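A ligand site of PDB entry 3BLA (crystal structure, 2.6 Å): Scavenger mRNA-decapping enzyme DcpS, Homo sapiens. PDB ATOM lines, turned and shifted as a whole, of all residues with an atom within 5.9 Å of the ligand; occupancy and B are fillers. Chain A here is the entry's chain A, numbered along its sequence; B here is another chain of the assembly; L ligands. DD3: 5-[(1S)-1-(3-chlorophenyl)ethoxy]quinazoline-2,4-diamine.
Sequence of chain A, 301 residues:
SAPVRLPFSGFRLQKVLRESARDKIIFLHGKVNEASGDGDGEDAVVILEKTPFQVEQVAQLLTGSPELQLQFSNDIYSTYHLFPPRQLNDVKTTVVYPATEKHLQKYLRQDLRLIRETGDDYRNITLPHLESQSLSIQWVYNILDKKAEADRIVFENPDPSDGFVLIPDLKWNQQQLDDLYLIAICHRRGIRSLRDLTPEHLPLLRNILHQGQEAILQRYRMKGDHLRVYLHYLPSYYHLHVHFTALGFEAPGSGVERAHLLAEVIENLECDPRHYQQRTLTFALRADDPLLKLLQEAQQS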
ATOM      1  N   ILE A  47     -31.750 -15.341 -10.673  1.00  0.00           N
ATOM      2  CA  ILE A  47     -33.030 -15.607 -10.057  1.00  0.00           C
ATOM      3  C   ILE A  47     -33.787 -14.291 -10.001  1.00  0.00           C
ATOM      4  O   ILE A  47     -33.246 -13.291  -9.549  1.00  0.00           O
ATOM      5  CB  ILE A  47     -32.874 -16.169  -8.615  1.00  0.00           C
ATOM      6  CG1 ILE A  47     -31.916 -17.368  -8.607  1.00  0.00           C
ATOM      7  CG2 ILE A  47     -34.224 -16.580  -8.052  1.00  0.00           C
ATOM      8  CD1 ILE A  47     -31.674 -17.925  -7.225  1.00  0.00           C
ATOM      9  N   THR A  94     -31.451 -11.897  -7.920  1.00  0.00           N
ATOM     10  CA  THR A  94     -30.230 -12.467  -7.352  1.00  0.00           C
ATOM     11  C   THR A  94     -29.432 -13.119  -8.476  1.00  0.00           C
ATOM     12  O   THR A  94     -30.007 -13.683  -9.401  1.00  0.00           O
ATOM     13  CB  THR A  94     -30.551 -13.491  -6.265  1.00  0.00           C
ATOM     14  OG1 THR A  94     -31.395 -12.885  -5.269  1.00  0.00           O
ATOM     15  CG2 THR A  94     -29.290 -13.992  -5.602  1.00  0.00           C
ATOM     16  N   VAL A  96     -25.907 -15.459  -9.588  1.00  0.00           N
ATOM     17  CA  VAL A  96     -24.822 -16.378  -9.251  1.00  0.00           C
ATOM     18  C   VAL A  96     -23.830 -16.421 -10.418  1.00  0.00           C
ATOM     19  O   VAL A  96     -24.171 -16.919 -11.495  1.00  0.00           O
ATOM     20  CB  VAL A  96     -25.327 -17.793  -8.992  1.00  0.00           C
ATOM     21  CG1 VAL A  96     -24.158 -18.746  -8.775  1.00  0.00           C
ATOM     22  CG2 VAL A  96     -26.268 -17.795  -7.787  1.00  0.00           C
ATOM     23  N   HIS A 103     -25.099 -25.611  -9.143  1.00  0.00           N
ATOM     24  CA  HIS A 103     -26.193 -24.643  -9.296  1.00  0.00           C
ATOM     25  C   HIS A 103     -27.130 -25.008 -10.438  1.00  0.00           C
ATOM     26  O   HIS A 103     -28.353 -25.024 -10.270  1.00  0.00           O
ATOM     27  CB  HIS A 103     -25.633 -23.237  -9.511  1.00  0.00           C
ATOM     28  CG  HIS A 103     -24.901 -22.700  -8.322  1.00  0.00           C
ATOM     29  ND1 HIS A 103     -23.523 -22.623  -8.257  1.00  0.00           N
ATOM     30  CD2 HIS A 103     -25.364 -22.201  -7.150  1.00  0.00           C
ATOM     31  CE1 HIS A 103     -23.168 -22.105  -7.101  1.00  0.00           C
ATOM     32  NE2 HIS A 103     -24.263 -21.848  -6.406  1.00  0.00           N
ATOM     33  N   LYS A 106     -29.142 -27.997  -9.471  1.00  0.00           N
ATOM     34  CA  LYS A 106     -29.869 -27.852  -8.188  1.00  0.00           C
ATOM     35  C   LYS A 106     -31.285 -27.318  -8.329  1.00  0.00           C
ATOM     36  O   LYS A 106     -32.156 -27.676  -7.539  1.00  0.00           O
ATOM     37  CB  LYS A 106     -29.060 -26.954  -7.227  1.00  0.00           C
ATOM     38  CG  LYS A 106     -29.790 -26.497  -5.957  1.00  0.00           C
ATOM     39  CD  LYS A 106     -28.862 -25.681  -5.059  1.00  0.00           C
ATOM     40  CE  LYS A 106     -29.606 -25.037  -3.892  1.00  0.00           C
ATOM     41  NZ  LYS A 106     -28.775 -23.994  -3.230  1.00  0.00           N
ATOM     42  N   TYR A 107     -31.509 -26.465  -9.314  1.00  0.00           N
ATOM     43  CA  TYR A 107     -32.772 -25.752  -9.453  1.00  0.00           C
ATOM     44  C   TYR A 107     -33.755 -26.412 -10.421  1.00  0.00           C
ATOM     45  O   TYR A 107     -34.970 -26.281 -10.240  1.00  0.00           O
ATOM     46  CB  TYR A 107     -32.515 -24.303  -9.860  1.00  0.00           C
ATOM     47  CG  TYR A 107     -31.626 -23.560  -8.882  1.00  0.00           C
ATOM     48  CD1 TYR A 107     -30.518 -22.843  -9.332  1.00  0.00           C
ATOM     49  CD2 TYR A 107     -31.875 -23.591  -7.512  1.00  0.00           C
ATOM     50  CE1 TYR A 107     -29.698 -22.165  -8.449  1.00  0.00           C
ATOM     51  CE2 TYR A 107     -31.064 -22.909  -6.615  1.00  0.00           C
ATOM     52  CZ  TYR A 107     -29.979 -22.201  -7.098  1.00  0.00           C
ATOM     53  OH  TYR A 107     -29.158 -21.532  -6.225  1.00  0.00           O
ATOM     54  N   TRP A 139     -19.563 -18.319   1.327  1.00  0.00           N
ATOM     55  CA  TRP A 139     -20.357 -17.150   1.701  1.00  0.00           C
ATOM     56  C   TRP A 139     -20.740 -17.140   3.179  1.00  0.00           C
ATOM     57  O   TRP A 139     -20.939 -16.070   3.767  1.00  0.00           O
ATOM     58  CB  TRP A 139     -21.620 -17.058   0.823  1.00  0.00           C
ATOM     59  CG  TRP A 139     -22.622 -18.142   1.071  1.00  0.00           C
ATOM     60  CD1 TRP A 139     -22.741 -19.316   0.391  1.00  0.00           C
ATOM     61  CD2 TRP A 139     -23.660 -18.150   2.078  1.00  0.00           C
ATOM     62  NE1 TRP A 139     -23.776 -20.056   0.900  1.00  0.00           N
ATOM     63  CE2 TRP A 139     -24.361 -19.361   1.927  1.00  0.00           C
ATOM     64  CE3 TRP A 139     -24.063 -17.250   3.070  1.00  0.00           C
ATOM     65  CZ2 TRP A 139     -25.453 -19.708   2.744  1.00  0.00           C
ATOM     66  CZ3 TRP A 139     -25.148 -17.592   3.883  1.00  0.00           C
ATOM     67  CH2 TRP A 139     -25.819 -18.817   3.721  1.00  0.00           C
ATOM     68  N   ILE A 143     -19.511 -14.286   6.058  1.00  0.00           N
ATOM     69  CA  ILE A 143     -20.305 -13.629   7.092  1.00  0.00           C
ATOM     70  C   ILE A 143     -19.649 -13.817   8.473  1.00  0.00           C
ATOM     71  O   ILE A 143     -19.568 -12.876   9.273  1.00  0.00           O
ATOM     72  CB  ILE A 143     -21.771 -14.167   7.096  1.00  0.00           C
ATOM     73  CG1 ILE A 143     -22.493 -13.749   5.805  1.00  0.00           C
ATOM     74  CG2 ILE A 143     -22.533 -13.660   8.297  1.00  0.00           C
ATOM     75  CD1 ILE A 143     -23.713 -14.588   5.452  1.00  0.00           C
ATOM     76  N   GLU A 149     -20.844  -8.789   4.081  1.00  0.00           N
ATOM     77  CA  GLU A 149     -22.115  -8.483   4.736  1.00  0.00           C
ATOM     78  C   GLU A 149     -21.982  -8.008   6.180  1.00  0.00           C
ATOM     79  O   GLU A 149     -22.994  -7.902   6.878  1.00  0.00           O
ATOM     80  CB  GLU A 149     -23.076  -9.668   4.661  1.00  0.00           C
ATOM     81  CG  GLU A 149     -23.254 -10.237   3.259  1.00  0.00           C
ATOM     82  CD  GLU A 149     -24.423 -11.207   3.184  1.00  0.00           C
ATOM     83  OE1 GLU A 149     -24.270 -12.330   2.665  1.00  0.00           O
ATOM     84  OE2 GLU A 149     -25.507 -10.844   3.632  1.00  0.00           O
ATOM     85  N   ARG A 152     -24.577  -5.714   7.607  1.00  0.00           N
ATOM     86  CA  ARG A 152     -25.958  -6.182   7.588  1.00  0.00           C
ATOM     87  C   ARG A 152     -26.243  -6.997   8.855  1.00  0.00           C
ATOM     88  O   ARG A 152     -27.396  -7.279   9.176  1.00  0.00           O
ATOM     89  CB  ARG A 152     -26.244  -7.064   6.367  1.00  0.00           C
ATOM     90  CG  ARG A 152     -25.947  -6.420   5.015  1.00  0.00           C
ATOM     91  CD  ARG A 152     -26.213  -7.386   3.871  1.00  0.00           C
ATOM     92  NE  ARG A 152     -27.644  -7.554   3.577  1.00  0.00           N
ATOM     93  CZ  ARG A 152     -28.404  -8.598   3.936  1.00  0.00           C
ATOM     94  NH1 ARG A 152     -27.920  -9.619   4.621  1.00  0.00           N
ATOM     95  NH2 ARG A 152     -29.691  -8.618   3.584  1.00  0.00           N
ATOM     96  N   ILE A 167     -28.580 -12.443  11.107  1.00  0.00           N
ATOM     97  CA  ILE A 167     -28.432 -11.682   9.861  1.00  0.00           C
ATOM     98  C   ILE A 167     -29.630 -11.989   8.967  1.00  0.00           C
ATOM     99  O   ILE A 167     -30.107 -13.129   8.963  1.00  0.00           O
ATOM    100  CB  ILE A 167     -27.089 -12.054   9.149  1.00  0.00           C
ATOM    101  CG1 ILE A 167     -26.841 -11.184   7.914  1.00  0.00           C
ATOM    102  CG2 ILE A 167     -27.055 -13.538   8.778  1.00  0.00           C
ATOM    103  CD1 ILE A 167     -25.395 -11.246   7.396  1.00  0.00           C
ATOM    104  N   PRO A 168     -30.147 -10.993   8.234  1.00  0.00           N
ATOM    105  CA  PRO A 168     -31.324 -11.311   7.420  1.00  0.00           C
ATOM    106  C   PRO A 168     -30.954 -12.285   6.309  1.00  0.00           C
ATOM    107  O   PRO A 168     -29.860 -12.195   5.761  1.00  0.00           O
ATOM    108  CB  PRO A 168     -31.732  -9.957   6.829  1.00  0.00           C
ATOM    109  CG  PRO A 168     -31.047  -8.939   7.666  1.00  0.00           C
ATOM    110  CD  PRO A 168     -29.770  -9.581   8.086  1.00  0.00           C
ATOM    111  N   ASP A 169     -31.845 -13.206   5.988  1.00  0.00           N
ATOM    112  CA  ASP A 169     -31.620 -14.089   4.853  1.00  0.00           C
ATOM    113  C   ASP A 169     -31.661 -13.272   3.551  1.00  0.00           C
ATOM    114  O   ASP A 169     -32.481 -12.370   3.397  1.00  0.00           O
ATOM    115  CB  ASP A 169     -32.684 -15.191   4.824  1.00  0.00           C
ATOM    116  CG  ASP A 169     -32.326 -16.317   3.867  1.00  0.00           C
ATOM    117  OD1 ASP A 169     -32.710 -16.226   2.675  1.00  0.00           O
ATOM    118  OD2 ASP A 169     -31.655 -17.285   4.289  1.00  0.00           O
ATOM    119  N   LEU A 170     -30.762 -13.592   2.619  1.00  0.00           N
ATOM    120  CA  LEU A 170     -30.765 -12.981   1.259  1.00  0.00           C
ATOM    121  C   LEU A 170     -32.163 -12.905   0.616  1.00  0.00           C
ATOM    122  O   LEU A 170     -32.474 -11.941  -0.071  1.00  0.00           O
ATOM    123  CB  LEU A 170     -29.722 -13.704   0.355  1.00  0.00           C
ATOM    124  CG  LEU A 170     -29.850 -14.072  -1.136  1.00  0.00           C
ATOM    125  CD1 LEU A 170     -30.774 -13.201  -1.953  1.00  0.00           C
ATOM    126  CD2 LEU A 170     -28.442 -14.068  -1.766  1.00  0.00           C
ATOM    127  N   LYS A 171     -33.002 -13.914   0.896  1.00  0.00           N
ATOM    128  CA  LYS A 171     -34.401 -13.978   0.444  1.00  0.00           C
ATOM    129  C   LYS A 171     -35.222 -12.741   0.811  1.00  0.00           C
ATOM    130  O   LYS A 171     -36.116 -12.341   0.067  1.00  0.00           O
ATOM    131  CB  LYS A 171     -35.069 -15.217   1.048  1.00  0.00           C
ATOM    132  CG  LYS A 171     -36.525 -15.490   0.634  1.00  0.00           C
ATOM    133  CD  LYS A 171     -36.629 -15.822  -0.838  1.00  0.00           C
ATOM    134  CE  LYS A 171     -37.893 -16.607  -1.178  1.00  0.00           C
ATOM    135  NZ  LYS A 171     -37.926 -16.919  -2.639  1.00  0.00           N
ATOM    136  N   ILE A 183     -31.506 -15.429   9.336  1.00  0.00           N
ATOM    137  CA  ILE A 183     -30.820 -16.665   9.695  1.00  0.00           C
ATOM    138  C   ILE A 183     -29.864 -16.407  10.830  1.00  0.00           C
ATOM    139  O   ILE A 183     -29.334 -15.289  10.956  1.00  0.00           O
ATOM    140  CB  ILE A 183     -30.080 -17.342   8.500  1.00  0.00           C
ATOM    141  CG1 ILE A 183     -29.253 -16.321   7.721  1.00  0.00           C
ATOM    142  CG2 ILE A 183     -31.074 -18.046   7.607  1.00  0.00           C
ATOM    143  CD1 ILE A 183     -28.489 -16.936   6.531  1.00  0.00           C
ATOM    144  N   SER A 236     -30.080 -26.686   3.092  1.00  0.00           N
ATOM    145  CA  SER A 236     -29.658 -26.368   1.735  1.00  0.00           C
ATOM    146  C   SER A 236     -28.156 -26.263   1.666  1.00  0.00           C
ATOM    147  O   SER A 236     -27.571 -26.426   0.601  1.00  0.00           O
ATOM    148  CB  SER A 236     -30.318 -25.075   1.270  1.00  0.00           C
ATOM    149  OG  SER A 236     -31.695 -25.275   1.088  1.00  0.00           O
ATOM    150  N   TYR A 237     -27.532 -25.978   2.811  1.00  0.00           N
ATOM    151  CA  TYR A 237     -26.069 -25.954   2.943  1.00  0.00           C
ATOM    152  C   TYR A 237     -25.686 -26.483   4.327  1.00  0.00           C
ATOM    153  O   TYR A 237     -26.429 -26.297   5.295  1.00  0.00           O
ATOM    154  CB  TYR A 237     -25.524 -24.554   2.713  1.00  0.00           C
ATOM    155  CG  TYR A 237     -26.272 -23.490   3.473  1.00  0.00           C
ATOM    156  CD1 TYR A 237     -25.806 -23.030   4.687  1.00  0.00           C
ATOM    157  CD2 TYR A 237     -27.448 -22.946   2.955  1.00  0.00           C
ATOM    158  CE1 TYR A 237     -26.491 -22.059   5.387  1.00  0.00           C
ATOM    159  CE2 TYR A 237     -28.150 -21.974   3.650  1.00  0.00           C
ATOM    160  CZ  TYR A 237     -27.660 -21.533   4.857  1.00  0.00           C
ATOM    161  OH  TYR A 237     -28.341 -20.561   5.565  1.00  0.00           O
ATOM    162  N   PHE B  72     -26.512  -5.984  -1.951  1.00  0.00           N
ATOM    163  CA  PHE B  72     -25.223  -6.424  -1.406  1.00  0.00           C
ATOM    164  C   PHE B  72     -24.642  -7.558  -2.250  1.00  0.00           C
ATOM    165  O   PHE B  72     -25.255  -8.008  -3.216  1.00  0.00           O
ATOM    166  CB  PHE B  72     -25.364  -6.869   0.063  1.00  0.00           C
ATOM    167  CG  PHE B  72     -26.298  -8.022   0.268  1.00  0.00           C
ATOM    168  CD1 PHE B  72     -25.808  -9.324   0.337  1.00  0.00           C
ATOM    169  CD2 PHE B  72     -27.668  -7.815   0.409  1.00  0.00           C
ATOM    170  CE1 PHE B  72     -26.673 -10.382   0.524  1.00  0.00           C
ATOM    171  CE2 PHE B  72     -28.537  -8.877   0.609  1.00  0.00           C
ATOM    172  CZ  PHE B  72     -28.043 -10.152   0.672  1.00  0.00           C
ATOM    173  N   ASN B  74     -21.697 -11.180  -1.915  1.00  0.00           N
ATOM    174  CA  ASN B  74     -20.942 -12.081  -1.055  1.00  0.00           C
ATOM    175  C   ASN B  74     -20.434 -13.192  -1.957  1.00  0.00           C
ATOM    176  O   ASN B  74     -21.232 -13.915  -2.549  1.00  0.00           O
ATOM    177  CB  ASN B  74     -21.851 -12.622   0.056  1.00  0.00           C
ATOM    178  CG  ASN B  74     -21.120 -13.502   1.056  1.00  0.00           C
ATOM    179  OD1 ASN B  74     -19.985 -13.904   0.832  1.00  0.00           O
ATOM    180  ND2 ASN B  74     -21.786 -13.804   2.167  1.00  0.00           N
ATOM    181  N   TYR B  77     -22.214 -14.444  -5.230  1.00  0.00           N
ATOM    182  CA  TYR B  77     -23.623 -14.074  -5.146  1.00  0.00           C
ATOM    183  C   TYR B  77     -23.763 -12.568  -5.027  1.00  0.00           C
ATOM    184  O   TYR B  77     -22.984 -11.923  -4.320  1.00  0.00           O
ATOM    185  CB  TYR B  77     -24.250 -14.718  -3.915  1.00  0.00           C
ATOM    186  CG  TYR B  77     -24.168 -16.225  -3.889  1.00  0.00           C
ATOM    187  CD1 TYR B  77     -23.149 -16.862  -3.183  1.00  0.00           C
ATOM    188  CD2 TYR B  77     -25.090 -17.001  -4.563  1.00  0.00           C
ATOM    189  CE1 TYR B  77     -23.065 -18.237  -3.150  1.00  0.00           C
ATOM    190  CE2 TYR B  77     -25.015 -18.379  -4.549  1.00  0.00           C
ATOM    191  CZ  TYR B  77     -24.002 -18.998  -3.831  1.00  0.00           C
ATOM    192  OH  TYR B  77     -23.911 -20.367  -3.803  1.00  0.00           O
HETATM  193  C14 DD3 L   1     -28.118 -19.237  -1.427  1.00  0.00           C
HETATM  194  C13 DD3 L   1     -28.889 -20.166   0.709  1.00  0.00           C
HETATM  195  C12 DD3 L   1     -27.872 -19.266   0.025  1.00  0.00           C
HETATM  196  C17 DD3 L   1     -28.554 -19.191  -4.189  1.00  0.00           C
HETATM  197  C16 DD3 L   1     -29.322 -18.392  -3.347  1.00  0.00           C
HETATM  198  C15 DD3 L   1     -29.106 -18.416  -1.970  1.00  0.00           C
HETATM  199  N3  DD3 L   1     -28.137 -14.851   3.503  1.00  0.00           N
HETATM  200  C10 DD3 L   1     -27.022 -16.993   0.550  1.00  0.00           C
HETATM  201  C8  DD3 L   1     -25.042 -15.894  -0.319  1.00  0.00           C
HETATM  202  C7  DD3 L   1     -25.096 -14.874   0.639  1.00  0.00           C
HETATM  203  C5  DD3 L   1     -27.119 -15.930   1.588  1.00  0.00           C
HETATM  204  C4  DD3 L   1     -28.175 -15.871   2.628  1.00  0.00           C
HETATM  205  C19 DD3 L   1     -27.353 -20.038  -2.279  1.00  0.00           C
HETATM  206  C9  DD3 L   1     -25.984 -16.926  -0.376  1.00  0.00           C
HETATM  207 CL2  DD3 L   1     -30.585 -17.347  -4.059  1.00  0.00          CL
HETATM  208  C18 DD3 L   1     -27.577 -20.020  -3.651  1.00  0.00           C
HETATM  209  O11 DD3 L   1     -27.997 -17.962   0.566  1.00  0.00           O
HETATM  210  C6  DD3 L   1     -26.101 -14.853   1.595  1.00  0.00           C
HETATM  211  N1  DD3 L   1     -26.184 -13.887   2.551  1.00  0.00           N
HETATM  212  N22 DD3 L   1     -29.165 -16.769   2.741  1.00  0.00           N
HETATM  213  C2  DD3 L   1     -27.188 -13.896   3.467  1.00  0.00           C
HETATM  214  N21 DD3 L   1     -27.278 -12.945   4.415  1.00  0.00           N
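A nitrogen (N1) of the ligand is in hydrogen-bond range of the side-chain carboxylate (OE1) of Glu 149. OD2 of Asp 169 is in hydrogen-bond range of N22 of the ligand (3.0 Å). The backbone carbonyl oxygen (O) of Pro 168 sits at hydrogen-bond distance from a nitrogen (N21) of the ligand. The backbone NH (N) of Leu 170 sits at hydrogen-bond distance from a nitrogen (N3) of the ligand, at 3.0 Å.
NH1 of Arg 152 is in salt-bridge range of OE2 of Glu 149. The side-chain amide nitrogen of Asn 74 of chain B sits at hydrogen-bond distance from the side-chain carboxylate of Glu 149 (2.9 Å). N of Lys 171 sits at hydrogen-bond distance from OD1 of Asp 169 (2.9 Å). The backbone carbonyl oxygen (O) of Pro 168 lies within hydrogen-bond range of the guanidinium group (NH1) of Arg 152 (3.4 Å). NE2 of His 103 is in hydrogen-bond range of OH of Tyr 77 of chain B (3.0 Å). The backbone NH (N) of Ile 47 sits at hydrogen-bond distance from the backbone carbonyl oxygen (O) of Thr 94 (2.7 Å). O of Trp 139 sits at hydrogen-bond distance from ND2 of Asn 74 of chain B, 2.9 Å away. The backbone NH (N) of Ile 183 is in hydrogen-bond range of the backbone carbonyl oxygen (O) of Ile 167.
The guanidinium group of Arg 152 sits close to a nitrogen (N21) of the ligand. Residues that only touch the ligand: Tyr 107 (3.2 Å), Tyr 77 of chain B (3.2 Å), Ile 47 (3.4 Å), Trp 139 (3.5 Å), Tyr 237 (3.5 Å), Ile 183 (3.7 Å), Asn 74 of chain B (3.8 Å), Ile 143 (3.9 Å), Thr 94 (3.9 Å) and Ile 167 (3.9 Å). Hydrophobic or aromatic side chains that line the ligand: Ile 47, Trp 139, Ile 143, Ile 167, Leu 170, Ile 183, Tyr 237 and Tyr 77 of chain B. Within 4 Å of the ligand: Ile 47, Thr 94, Tyr 107, Trp 139, Ile 143, Glu 149, Arg 152, Ile 167, Pro 168, Asp 169, Leu 170, Ile 183, Tyr 237, Asn 74 of chain B and Tyr 77 of chain B. The nearest printed residue that does not touch the ligand is Phe 72 of chain B (4.1 Å).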
